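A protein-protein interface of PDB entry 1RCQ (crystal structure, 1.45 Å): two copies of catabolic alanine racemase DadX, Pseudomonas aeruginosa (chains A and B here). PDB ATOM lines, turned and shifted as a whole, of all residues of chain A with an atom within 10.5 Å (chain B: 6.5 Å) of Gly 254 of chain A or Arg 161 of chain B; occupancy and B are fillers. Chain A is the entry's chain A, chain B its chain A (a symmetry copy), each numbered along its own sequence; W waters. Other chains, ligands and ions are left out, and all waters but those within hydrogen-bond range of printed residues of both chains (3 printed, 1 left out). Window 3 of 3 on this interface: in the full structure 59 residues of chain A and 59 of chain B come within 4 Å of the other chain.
Of chain A, only Gly 254 (3.8 Å) comes within 4 Å of Arg 161 of chain B.
Ser 160 of chain B touches three residues of chain A.
No residue of chain A comes within 4 Å of Ala 162 of chain B.
No residue of chain A comes within 4 Å of Asp 163 of chain B.
No residue of chain A comes within 4 Å of Glu 164 of chain B.
No residue of chain A comes within 4 Å of Cys 167 of chain B.
Of the printed residues of chain B, Pro 250 of chain A touches Met 127 (3.6 Å) and Arg 169 (3.6 Å).
Printed residues of chain B within 4 Å of Tyr 253 of chain A: Met 127, Phe 159 and Ser 160.
Tyr 257 of chain A touches none of the printed residues of chain B.
The nearest residue of chain B that does not touch Gly 254 of chain A is Glu 164 of chain B (4.2 Å).
The nearest residue of chain A that does not touch Arg 161 of chain B is Ala 255 of chain A (4.1 Å).
The backbone NH (N) of Gly 254 of chain A is in hydrogen-bond range of the backbone carbonyl oxygen (O) of Ser 160 of chain B.
The backbone carbonyl oxygen (O) of Met 127 of chain B sits at hydrogen-bond distance from the backbone NH (N) of Gly 252 of chain A.
Hydrophobic or aromatic side chains of chain A that line the printed part of chain B: Pro 250 and Tyr 253.
Among the printed residues, 10 pairs touch across the chains.
Among the printed residues, no Asp or Glu carboxylate lies within 4 Å of a Lys or Arg side-chain nitrogen of the other chain.
O of Pro 250 of chain A touches O of Met 127 of chain B, 3.6 Å away.
Arg 169 of chain B touches Pro 250 of chain A (NH2 to CG, 3.6 Å).
CA of Val 251 of chain A touches O of Met 127 of chain B (3.8 Å).
Gly 252 of chain A touches Ser 160 of chain B.
Met 127 of chain B touches Tyr 253 of chain A.
O of Phe 159 of chain B touches CE1 of Tyr 253 of chain A, 3.6 Å away.
CA of Tyr 253 of chain A touches O of Ser 160 of chain B, 3.3 Å away.
Arg 161 of chain B touches Gly 254 of chain A (CG to N, 3.8 Å).
No position is printed for both chains.
Of the 10 pairs that touch across the chains among the printed residues, none has its exchanged pair printed and touching as well.
Water W3 lies within hydrogen-bond range of the guanidinium group of Arg 169 of chain B (2.7 Å) and the side-chain carboxylate of Glu 249 of chain A (2.8 Å).
Water W1 bridges the side-chain amide nitrogen of Asn 192 of chain B (2.9 Å) and the side-chain hydroxyl of Tyr 253 of chain A (3.0 Å).
Water W2 bridges O of Gly 254 of chain A and OE2 of Glu 164 of chain B.
The side-chain sulfur of Cys 167 of chain B sits close to the backbone NH of Arg 169 of chain B, at 3.5 Å.
The side-chain carboxylate of Glu 164 of chain B lies within salt-bridge range of the guanidinium group of Arg 161 of chain B (2.8 Å).
The backbone NH (N) of Ser 160 of chain B is in hydrogen-bond range of the side-chain amide oxygen (OE1) of Gln 173 of chain B, 3.0 Å away.
The guanidinium group of Arg 161 of chain B sits close to the side-chain sulfur of Cys 167 of chain B (3.6 Å).
NE2 of Gln 173 of chain B lies close to N of Met 127 of chain B (3.4 Å).
O of Tyr 257 of chain A sits at hydrogen-bond distance from N of Val 251 of chain A (2.8 Å).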
ATOM      1  N   GLY A 248      13.978   6.790  12.865  1.00  0.00           N
ATOM      2  CA  GLY A 248      14.834   5.722  13.287  1.00  0.00           C
ATOM      3  C   GLY A 248      14.355   5.042  14.542  1.00  0.00           C
ATOM      4  O   GLY A 248      15.188   4.470  15.255  1.00  0.00           O
ATOM      5  N   GLU A 249      13.059   5.105  14.819  1.00  0.00           N
ATOM      6  CA  GLU A 249      12.492   4.512  16.013  1.00  0.00           C
ATOM      7  C   GLU A 249      11.781   3.203  15.635  1.00  0.00           C
ATOM      8  O   GLU A 249      11.009   3.175  14.688  1.00  0.00           O
ATOM      9  CB  GLU A 249      11.509   5.444  16.702  1.00  0.00           C
ATOM     10  CG  GLU A 249      12.209   6.642  17.340  1.00  0.00           C
ATOM     11  CD  GLU A 249      13.012   6.222  18.556  1.00  0.00           C
ATOM     12  OE1 GLU A 249      12.614   5.291  19.303  1.00  0.00           O
ATOM     13  OE2 GLU A 249      14.089   6.841  18.771  1.00  0.00           O
ATOM     14  N   PRO A 250      12.080   2.153  16.375  1.00  0.00           N
ATOM     15  CA  PRO A 250      11.534   0.831  16.080  1.00  0.00           C
ATOM     16  C   PRO A 250      10.066   0.753  16.484  1.00  0.00           C
ATOM     17  O   PRO A 250       9.700   1.280  17.545  1.00  0.00           O
ATOM     18  CB  PRO A 250      12.392  -0.117  16.941  1.00  0.00           C
ATOM     19  CG  PRO A 250      12.793   0.726  18.104  1.00  0.00           C
ATOM     20  CD  PRO A 250      12.963   2.120  17.558  1.00  0.00           C
ATOM     21  N   VAL A 251       9.262   0.136  15.639  1.00  0.00           N
ATOM     22  CA  VAL A 251       7.841   0.003  15.951  1.00  0.00           C
ATOM     23  C   VAL A 251       7.455  -1.473  16.072  1.00  0.00           C
ATOM     24  O   VAL A 251       7.583  -2.236  15.116  1.00  0.00           O
ATOM     25  CB  VAL A 251       6.961   0.663  14.894  1.00  0.00           C
ATOM     26  CG1 VAL A 251       5.485   0.607  15.310  1.00  0.00           C
ATOM     27  CG2 VAL A 251       7.391   2.108  14.657  1.00  0.00           C
ATOM     28  N   GLY A 252       6.974  -1.879  17.242  1.00  0.00           N
ATOM     29  CA  GLY A 252       6.450  -3.198  17.518  1.00  0.00           C
ATOM     30  C   GLY A 252       7.508  -4.197  17.922  1.00  0.00           C
ATOM     31  O   GLY A 252       8.693  -3.907  18.022  1.00  0.00           O
ATOM     32  N   TYR A 253       7.077  -5.425  18.154  1.00  0.00           N
ATOM     33  CA  TYR A 253       7.989  -6.492  18.470  1.00  0.00           C
ATOM     34  C   TYR A 253       9.038  -6.664  17.384  1.00  0.00           C
ATOM     35  O   TYR A 253       8.790  -6.536  16.178  1.00  0.00           O
ATOM     36  CB  TYR A 253       7.196  -7.791  18.588  1.00  0.00           C
ATOM     37  CG  TYR A 253       6.302  -7.989  19.760  1.00  0.00           C
ATOM     38  CD1 TYR A 253       6.796  -7.925  21.062  1.00  0.00           C
ATOM     39  CD2 TYR A 253       4.960  -8.269  19.528  1.00  0.00           C
ATOM     40  CE1 TYR A 253       5.969  -8.116  22.154  1.00  0.00           C
ATOM     41  CE2 TYR A 253       4.131  -8.462  20.609  1.00  0.00           C
ATOM     42  CZ  TYR A 253       4.653  -8.380  21.884  1.00  0.00           C
ATOM     43  OH  TYR A 253       3.805  -8.588  22.932  1.00  0.00           O
ATOM     44  N   GLY A 254      10.240  -7.036  17.784  1.00  0.00           N
ATOM     45  CA  GLY A 254      11.300  -7.382  16.835  1.00  0.00           C
ATOM     46  C   GLY A 254      11.900  -6.198  16.113  1.00  0.00           C
ATOM     47  O   GLY A 254      12.894  -6.396  15.401  1.00  0.00           O
ATOM     48  N   ALA A 255      11.352  -5.018  16.278  1.00  0.00           N
ATOM     49  CA  ALA A 255      11.833  -3.865  15.494  1.00  0.00           C
ATOM     50  C   ALA A 255      12.045  -4.160  14.009  1.00  0.00           C
ATOM     51  O   ALA A 255      13.031  -3.730  13.408  1.00  0.00           O
ATOM     52  CB  ALA A 255      13.139  -3.331  16.087  1.00  0.00           C
ATOM     53  N   ARG A 256      11.172  -4.946  13.377  1.00  0.00           N
ATOM     54  CA  ARG A 256      11.301  -5.196  11.940  1.00  0.00           C
ATOM     55  C   ARG A 256      11.233  -3.909  11.141  1.00  0.00           C
ATOM     56  O   ARG A 256      11.879  -3.676  10.129  1.00  0.00           O
ATOM     57  CB  ARG A 256      10.143  -6.108  11.518  1.00  0.00           C
ATOM     58  CG  ARG A 256      10.135  -6.421  10.034  1.00  0.00           C
ATOM     59  CD  ARG A 256       8.896  -7.201   9.579  1.00  0.00           C
ATOM     60  NE  ARG A 256       7.721  -6.330   9.501  1.00  0.00           N
ATOM     61  CZ  ARG A 256       6.488  -6.783   9.365  1.00  0.00           C
ATOM     62  NH1 ARG A 256       6.242  -8.082   9.305  1.00  0.00           N
ATOM     63  NH2 ARG A 256       5.487  -5.926   9.311  1.00  0.00           N
ATOM     64  N   TYR A 257      10.389  -3.009  11.626  1.00  0.00           N
ATOM     65  CA  TYR A 257      10.232  -1.665  11.084  1.00  0.00           C
ATOM     66  C   TYR A 257      10.775  -0.586  12.014  1.00  0.00           C
ATOM     67  O   TYR A 257      10.519  -0.597  13.219  1.00  0.00           O
ATOM     68  CB  TYR A 257       8.732  -1.394  10.805  1.00  0.00           C
ATOM     69  CG  TYR A 257       8.500  -0.016  10.240  1.00  0.00           C
ATOM     70  CD1 TYR A 257       8.723   0.163   8.877  1.00  0.00           C
ATOM     71  CD2 TYR A 257       8.091   1.065  11.014  1.00  0.00           C
ATOM     72  CE1 TYR A 257       8.540   1.381   8.278  1.00  0.00           C
ATOM     73  CE2 TYR A 257       7.905   2.307  10.419  1.00  0.00           C
ATOM     74  CZ  TYR A 257       8.125   2.447   9.058  1.00  0.00           C
ATOM     75  OH  TYR A 257       7.955   3.682   8.470  1.00  0.00           O
ATOM     76  N   SER A 258      11.537   0.325  11.438  1.00  0.00           N
ATOM     77  CA  SER A 258      11.919   1.587  12.082  1.00  0.00           C
ATOM     78  C   SER A 258      11.377   2.768  11.293  1.00  0.00           C
ATOM     79  O   SER A 258      11.337   2.700  10.054  1.00  0.00           O
ATOM     80  CB  SER A 258      13.437   1.688  12.235  1.00  0.00           C
ATOM     81  OG  SER A 258      13.741   0.795  13.302  1.00  0.00           O
ATOM     82  N   ARG A 278      -0.123 -12.116  10.703  1.00  0.00           N
ATOM     83  CA  ARG A 278       1.138 -11.690  11.303  1.00  0.00           C
ATOM     84  C   ARG A 278       2.242 -11.534  10.268  1.00  0.00           C
ATOM     85  O   ARG A 278       3.185 -10.776  10.452  1.00  0.00           O
ATOM     86  CB  ARG A 278       1.584 -12.660  12.395  1.00  0.00           C
ATOM     87  CG  ARG A 278       2.802 -12.148  13.172  1.00  0.00           C
ATOM     88  CD  ARG A 278       3.321 -13.180  14.155  1.00  0.00           C
ATOM     89  NE  ARG A 278       4.608 -12.753  14.688  1.00  0.00           N
ATOM     90  CZ  ARG A 278       5.811 -13.067  14.199  1.00  0.00           C
ATOM     91  NH1 ARG A 278       5.969 -13.840  13.129  1.00  0.00           N
ATOM     92  NH2 ARG A 278       6.897 -12.596  14.803  1.00  0.00           N
ATOM     93  N   ASP A 282       5.690  -4.678   6.140  1.00  0.00           N
ATOM     94  CA  ASP A 282       5.598  -3.226   6.110  1.00  0.00           C
ATOM     95  C   ASP A 282       5.314  -2.804   4.675  1.00  0.00           C
ATOM     96  O   ASP A 282       5.949  -3.295   3.746  1.00  0.00           O
ATOM     97  CB  ASP A 282       6.898  -2.636   6.629  1.00  0.00           C
ATOM     98  CG  ASP A 282       7.223  -3.161   8.025  1.00  0.00           C
ATOM     99  OD1 ASP A 282       6.325  -3.143   8.885  1.00  0.00           O
ATOM    100  OD2 ASP A 282       8.356  -3.622   8.259  1.00  0.00           O
ATOM    101  N   GLY A 297       5.268  -1.844  10.994  1.00  0.00           N
ATOM    102  CA  GLY A 297       5.518  -2.560  12.204  1.00  0.00           C
ATOM    103  C   GLY A 297       4.827  -3.905  12.240  1.00  0.00           C
ATOM    104  O   GLY A 297       3.761  -4.154  11.671  1.00  0.00           O
ATOM    105  N   ARG A 298       5.480  -4.815  12.962  1.00  0.00           N
ATOM    106  CA  ARG A 298       4.928  -6.149  13.114  1.00  0.00           C
ATOM    107  C   ARG A 298       3.583  -6.156  13.831  1.00  0.00           C
ATOM    108  O   ARG A 298       3.386  -5.527  14.874  1.00  0.00           O
ATOM    109  CB  ARG A 298       5.918  -7.013  13.897  1.00  0.00           C
ATOM    110  CG  ARG A 298       5.517  -8.428  14.186  1.00  0.00           C
ATOM    111  CD  ARG A 298       5.489  -9.316  12.969  1.00  0.00           C
ATOM    112  NE  ARG A 298       6.850  -9.705  12.608  1.00  0.00           N
ATOM    113  CZ  ARG A 298       7.048 -10.598  11.626  1.00  0.00           C
ATOM    114  NH1 ARG A 298       6.033 -11.127  10.986  1.00  0.00           N
ATOM    115  NH2 ARG A 298       8.280 -10.950  11.305  1.00  0.00           N
ATOM    116  N   VAL A 299       2.659  -6.901  13.221  1.00  0.00           N
ATOM    117  CA  VAL A 299       1.363  -7.172  13.806  1.00  0.00           C
ATOM    118  C   VAL A 299       1.500  -7.962  15.100  1.00  0.00           C
ATOM    119  O   VAL A 299       2.248  -8.951  15.140  1.00  0.00           O
ATOM    120  CB  VAL A 299       0.520  -7.951  12.774  1.00  0.00           C
ATOM    121  CG1 VAL A 299      -0.786  -8.450  13.388  1.00  0.00           C
ATOM    122  CG2 VAL A 299       0.206  -7.083  11.573  1.00  0.00           C
ATOM    123  N   SER A 300       0.815  -7.535  16.146  1.00  0.00           N
ATOM    124  CA  SER A 300       0.735  -8.176  17.443  1.00  0.00           C
ATOM    125  C   SER A 300      -0.535  -9.035  17.526  1.00  0.00           C
ATOM    126  O   SER A 300      -1.372  -9.130  16.615  1.00  0.00           O
ATOM    127  CB  SER A 300       0.719  -7.106  18.550  1.00  0.00           C
ATOM    128  OG  SER A 300       1.923  -6.367  18.654  1.00  0.00           O
ATOM    129  N   MET B 127       8.971   0.251  22.746  1.00  0.00           N
ATOM    130  CA  MET B 127       8.333  -0.616  21.756  1.00  0.00           C
ATOM    131  C   MET B 127       7.468   0.213  20.823  1.00  0.00           C
ATOM    132  O   MET B 127       7.239  -0.170  19.673  1.00  0.00           O
ATOM    133  CB  MET B 127       7.493  -1.699  22.428  1.00  0.00           C
ATOM    134  CG  MET B 127       6.783  -2.651  21.428  1.00  0.00           C
ATOM    135  SD  MET B 127       6.167  -4.041  22.393  1.00  0.00           S
ATOM    136  CE  MET B 127       5.195  -4.893  21.166  1.00  0.00           C
ATOM    137  N   PHE B 159       8.138  -5.038  26.763  1.00  0.00           N
ATOM    138  CA  PHE B 159       9.354  -5.193  25.997  1.00  0.00           C
ATOM    139  C   PHE B 159       9.112  -5.642  24.562  1.00  0.00           C
ATOM    140  O   PHE B 159       8.308  -6.507  24.306  1.00  0.00           O
ATOM    141  CB  PHE B 159      10.303  -6.216  26.643  1.00  0.00           C
ATOM    142  CG  PHE B 159      10.768  -5.810  28.028  1.00  0.00           C
ATOM    143  CD1 PHE B 159      11.486  -4.628  28.198  1.00  0.00           C
ATOM    144  CD2 PHE B 159      10.493  -6.583  29.139  1.00  0.00           C
ATOM    145  CE1 PHE B 159      11.930  -4.234  29.449  1.00  0.00           C
ATOM    146  CE2 PHE B 159      10.922  -6.200  30.388  1.00  0.00           C
ATOM    147  CZ  PHE B 159      11.616  -5.022  30.543  1.00  0.00           C
ATOM    148  N   SER B 160       9.864  -5.097  23.631  1.00  0.00           N
ATOM    149  CA  SER B 160       9.725  -5.466  22.249  1.00  0.00           C
ATOM    150  C   SER B 160      10.580  -6.642  21.834  1.00  0.00           C
ATOM    151  O   SER B 160      10.182  -7.266  20.845  1.00  0.00           O
ATOM    152  CB  SER B 160      10.131  -4.275  21.362  1.00  0.00           C
ATOM    153  OG  SER B 160      11.429  -3.866  21.712  1.00  0.00           O
ATOM    154  N   ARG B 161      11.691  -6.885  22.512  1.00  0.00           N
ATOM    155  CA  ARG B 161      12.676  -7.831  22.009  1.00  0.00           C
ATOM    156  C   ARG B 161      13.244  -8.700  23.114  1.00  0.00           C
ATOM    157  O   ARG B 161      14.423  -9.089  23.013  1.00  0.00           O
ATOM    158  CB  ARG B 161      13.793  -7.051  21.294  1.00  0.00           C
ATOM    159  CG  ARG B 161      13.311  -6.392  19.999  1.00  0.00           C
ATOM    160  CD  ARG B 161      14.403  -5.603  19.270  1.00  0.00           C
ATOM    161  NE  ARG B 161      15.278  -6.495  18.503  1.00  0.00           N
ATOM    162  CZ  ARG B 161      16.366  -6.066  17.882  1.00  0.00           C
ATOM    163  NH1 ARG B 161      16.664  -4.769  17.967  1.00  0.00           N
ATOM    164  NH2 ARG B 161      17.147  -6.894  17.192  1.00  0.00           N
ATOM    165  N   ALA B 162      12.453  -8.983  24.149  1.00  0.00           N
ATOM    166  CA  ALA B 162      13.044  -9.761  25.250  1.00  0.00           C
ATOM    167  C   ALA B 162      13.283 -11.214  24.844  1.00  0.00           C
ATOM    168  O   ALA B 162      14.022 -11.929  25.516  1.00  0.00           O
ATOM    169  CB  ALA B 162      12.193  -9.636  26.503  1.00  0.00           C
ATOM    170  N   ASP B 163      12.689 -11.663  23.734  1.00  0.00           N
ATOM    171  CA  ASP B 163      12.930 -12.995  23.231  1.00  0.00           C
ATOM    172  C   ASP B 163      14.318 -13.063  22.578  1.00  0.00           C
ATOM    173  O   ASP B 163      14.742 -14.191  22.282  1.00  0.00           O
ATOM    174  CB  ASP B 163      11.897 -13.465  22.208  1.00  0.00           C
ATOM    175  CG  ASP B 163      11.808 -12.533  21.030  1.00  0.00           C
ATOM    176  OD1 ASP B 163      11.739 -11.296  21.227  1.00  0.00           O
ATOM    177  OD2 ASP B 163      11.783 -13.042  19.888  1.00  0.00           O
ATOM    178  N   GLU B 164      14.976 -11.936  22.370  1.00  0.00           N
ATOM    179  CA  GLU B 164      16.343 -11.898  21.811  1.00  0.00           C
ATOM    180  C   GLU B 164      17.353 -11.665  22.933  1.00  0.00           C
ATOM    181  O   GLU B 164      17.625 -10.558  23.379  1.00  0.00           O
ATOM    182  CB  GLU B 164      16.437 -10.857  20.721  1.00  0.00           C
ATOM    183  CG  GLU B 164      15.581 -11.131  19.484  1.00  0.00           C
ATOM    184  CD  GLU B 164      15.736  -9.969  18.514  1.00  0.00           C
ATOM    185  OE1 GLU B 164      16.853  -9.823  17.977  1.00  0.00           O
ATOM    186  OE2 GLU B 164      14.739  -9.240  18.345  1.00  0.00           O
ATOM    187  N   LEU B 165      17.880 -12.793  23.403  1.00  0.00           N
ATOM    188  CA  LEU B 165      18.711 -12.777  24.590  1.00  0.00           C
ATOM    189  C   LEU B 165      20.050 -12.063  24.457  1.00  0.00           C
ATOM    190  O   LEU B 165      20.666 -11.714  25.464  1.00  0.00           O
ATOM    191  CB  LEU B 165      18.923 -14.245  25.021  1.00  0.00           C
ATOM    192  CG  LEU B 165      17.634 -14.915  25.521  1.00  0.00           C
ATOM    193  CD1 LEU B 165      17.839 -16.410  25.728  1.00  0.00           C
ATOM    194  CD2 LEU B 165      17.114 -14.269  26.809  1.00  0.00           C
ATOM    195  N   CYS B 167      20.307  -9.332  22.500  1.00  0.00           N
ATOM    196  CA  CYS B 167      19.934  -7.967  22.146  1.00  0.00           C
ATOM    197  C   CYS B 167      19.774  -7.084  23.377  1.00  0.00           C
ATOM    198  O   CYS B 167      19.031  -7.418  24.308  1.00  0.00           O
ATOM    199  CB  CYS B 167      18.638  -7.976  21.312  1.00  0.00           C
ATOM    200  SG  CYS B 167      17.989  -6.348  20.904  1.00  0.00           S
ATOM    201  N   ARG B 169      18.122  -4.379  23.776  1.00  0.00           N
ATOM    202  CA  ARG B 169      16.942  -3.487  23.780  1.00  0.00           C
ATOM    203  C   ARG B 169      16.199  -3.531  25.099  1.00  0.00           C
ATOM    204  O   ARG B 169      15.675  -2.520  25.602  1.00  0.00           O
ATOM    205  CB  ARG B 169      16.012  -3.812  22.599  1.00  0.00           C
ATOM    206  CG  ARG B 169      14.846  -2.846  22.467  1.00  0.00           C
ATOM    207  CD  ARG B 169      15.319  -1.412  22.399  1.00  0.00           C
ATOM    208  NE  ARG B 169      14.270  -0.507  21.979  1.00  0.00           N
ATOM    209  CZ  ARG B 169      14.418   0.814  21.954  1.00  0.00           C
ATOM    210  NH1 ARG B 169      15.584   1.302  22.355  1.00  0.00           N
ATOM    211  NH2 ARG B 169      13.395   1.558  21.540  1.00  0.00           N
ATOM    212  N   THR B 170      16.153  -4.709  25.702  1.00  0.00           N
ATOM    213  CA  THR B 170      15.457  -4.887  26.984  1.00  0.00           C
ATOM    214  C   THR B 170      16.096  -4.038  28.072  1.00  0.00           C
ATOM    215  O   THR B 170      15.415  -3.397  28.873  1.00  0.00           O
ATOM    216  CB  THR B 170      15.425  -6.388  27.339  1.00  0.00           C
ATOM    217  OG1 THR B 170      14.654  -7.075  26.332  1.00  0.00           O
ATOM    218  CG2 THR B 170      14.767  -6.586  28.687  1.00  0.00           C
ATOM    219  N   GLN B 173      15.168  -0.299  27.403  1.00  0.00           N
ATOM    220  CA  GLN B 173      13.798  -0.017  27.791  1.00  0.00           C
ATOM    221  C   GLN B 173      13.705   0.043  29.306  1.00  0.00           C
ATOM    222  O   GLN B 173      13.031   0.943  29.804  1.00  0.00           O
ATOM    223  CB  GLN B 173      12.820  -1.044  27.250  1.00  0.00           C
ATOM    224  CG  GLN B 173      12.609  -1.077  25.751  1.00  0.00           C
ATOM    225  CD  GLN B 173      11.484  -2.012  25.317  1.00  0.00           C
ATOM    226  OE1 GLN B 173      11.700  -3.159  24.916  1.00  0.00           O
ATOM    227  NE2 GLN B 173      10.241  -1.529  25.374  1.00  0.00           N
ATOM    228  N   ASN B 192       7.130  -9.945  30.637  1.00  0.00           N
ATOM    229  CA  ASN B 192       6.422 -10.955  29.861  1.00  0.00           C
ATOM    230  C   ASN B 192       7.190 -12.269  29.935  1.00  0.00           C
ATOM    231  O   ASN B 192       8.169 -12.314  30.707  1.00  0.00           O
ATOM    232  CB  ASN B 192       6.242 -10.494  28.415  1.00  0.00           C
ATOM    233  CG  ASN B 192       7.583 -10.295  27.706  1.00  0.00           C
ATOM    234  OD1 ASN B 192       8.649 -10.377  28.305  1.00  0.00           O
ATOM    235  ND2 ASN B 192       7.552 -10.013  26.392  1.00  0.00           N
ATOM    236  N   PRO B 194       9.364 -14.025  27.870  1.00  0.00           N
ATOM    237  CA  PRO B 194      10.827 -14.047  27.680  1.00  0.00           C
ATOM    238  C   PRO B 194      11.579 -13.308  28.769  1.00  0.00           C
ATOM    239  O   PRO B 194      12.673 -13.764  29.124  1.00  0.00           O
ATOM    240  CB  PRO B 194      11.003 -13.372  26.321  1.00  0.00           C
ATOM    241  CG  PRO B 194       9.717 -12.658  26.052  1.00  0.00           C
ATOM    242  CD  PRO B 194       8.647 -13.482  26.702  1.00  0.00           C
ATOM    243  N   TRP B 199      15.568 -12.874  31.655  1.00  0.00           N
ATOM    244  CA  TRP B 199      16.154 -11.589  32.038  1.00  0.00           C
ATOM    245  C   TRP B 199      16.038 -11.326  33.535  1.00  0.00           C
ATOM    246  O   TRP B 199      15.271 -10.481  33.983  1.00  0.00           O
ATOM    247  CB  TRP B 199      15.478 -10.469  31.261  1.00  0.00           C
ATOM    248  CG  TRP B 199      15.750 -10.490  29.790  1.00  0.00           C
ATOM    249  CD1 TRP B 199      15.125 -11.182  28.809  1.00  0.00           C
ATOM    250  CD2 TRP B 199      16.789  -9.735  29.130  1.00  0.00           C
ATOM    251  NE1 TRP B 199      15.674 -10.922  27.596  1.00  0.00           N
ATOM    252  CE2 TRP B 199      16.704 -10.035  27.754  1.00  0.00           C
ATOM    253  CE3 TRP B 199      17.756  -8.845  29.608  1.00  0.00           C
ATOM    254  CZ2 TRP B 199      17.569  -9.463  26.835  1.00  0.00           C
ATOM    255  CZ3 TRP B 199      18.617  -8.278  28.687  1.00  0.00           C
ATOM    256  CH2 TRP B 199      18.516  -8.593  27.322  1.00  0.00           C
HETATM  257  O   HOH W   1       5.574 -10.611  24.372  1.00  0.00           O
HETATM  258  O   HOH W   2      14.251  -9.040  15.302  1.00  0.00           O
HETATM  259  O   HOH W   3      13.639   4.278  21.646  1.00  0.00           O
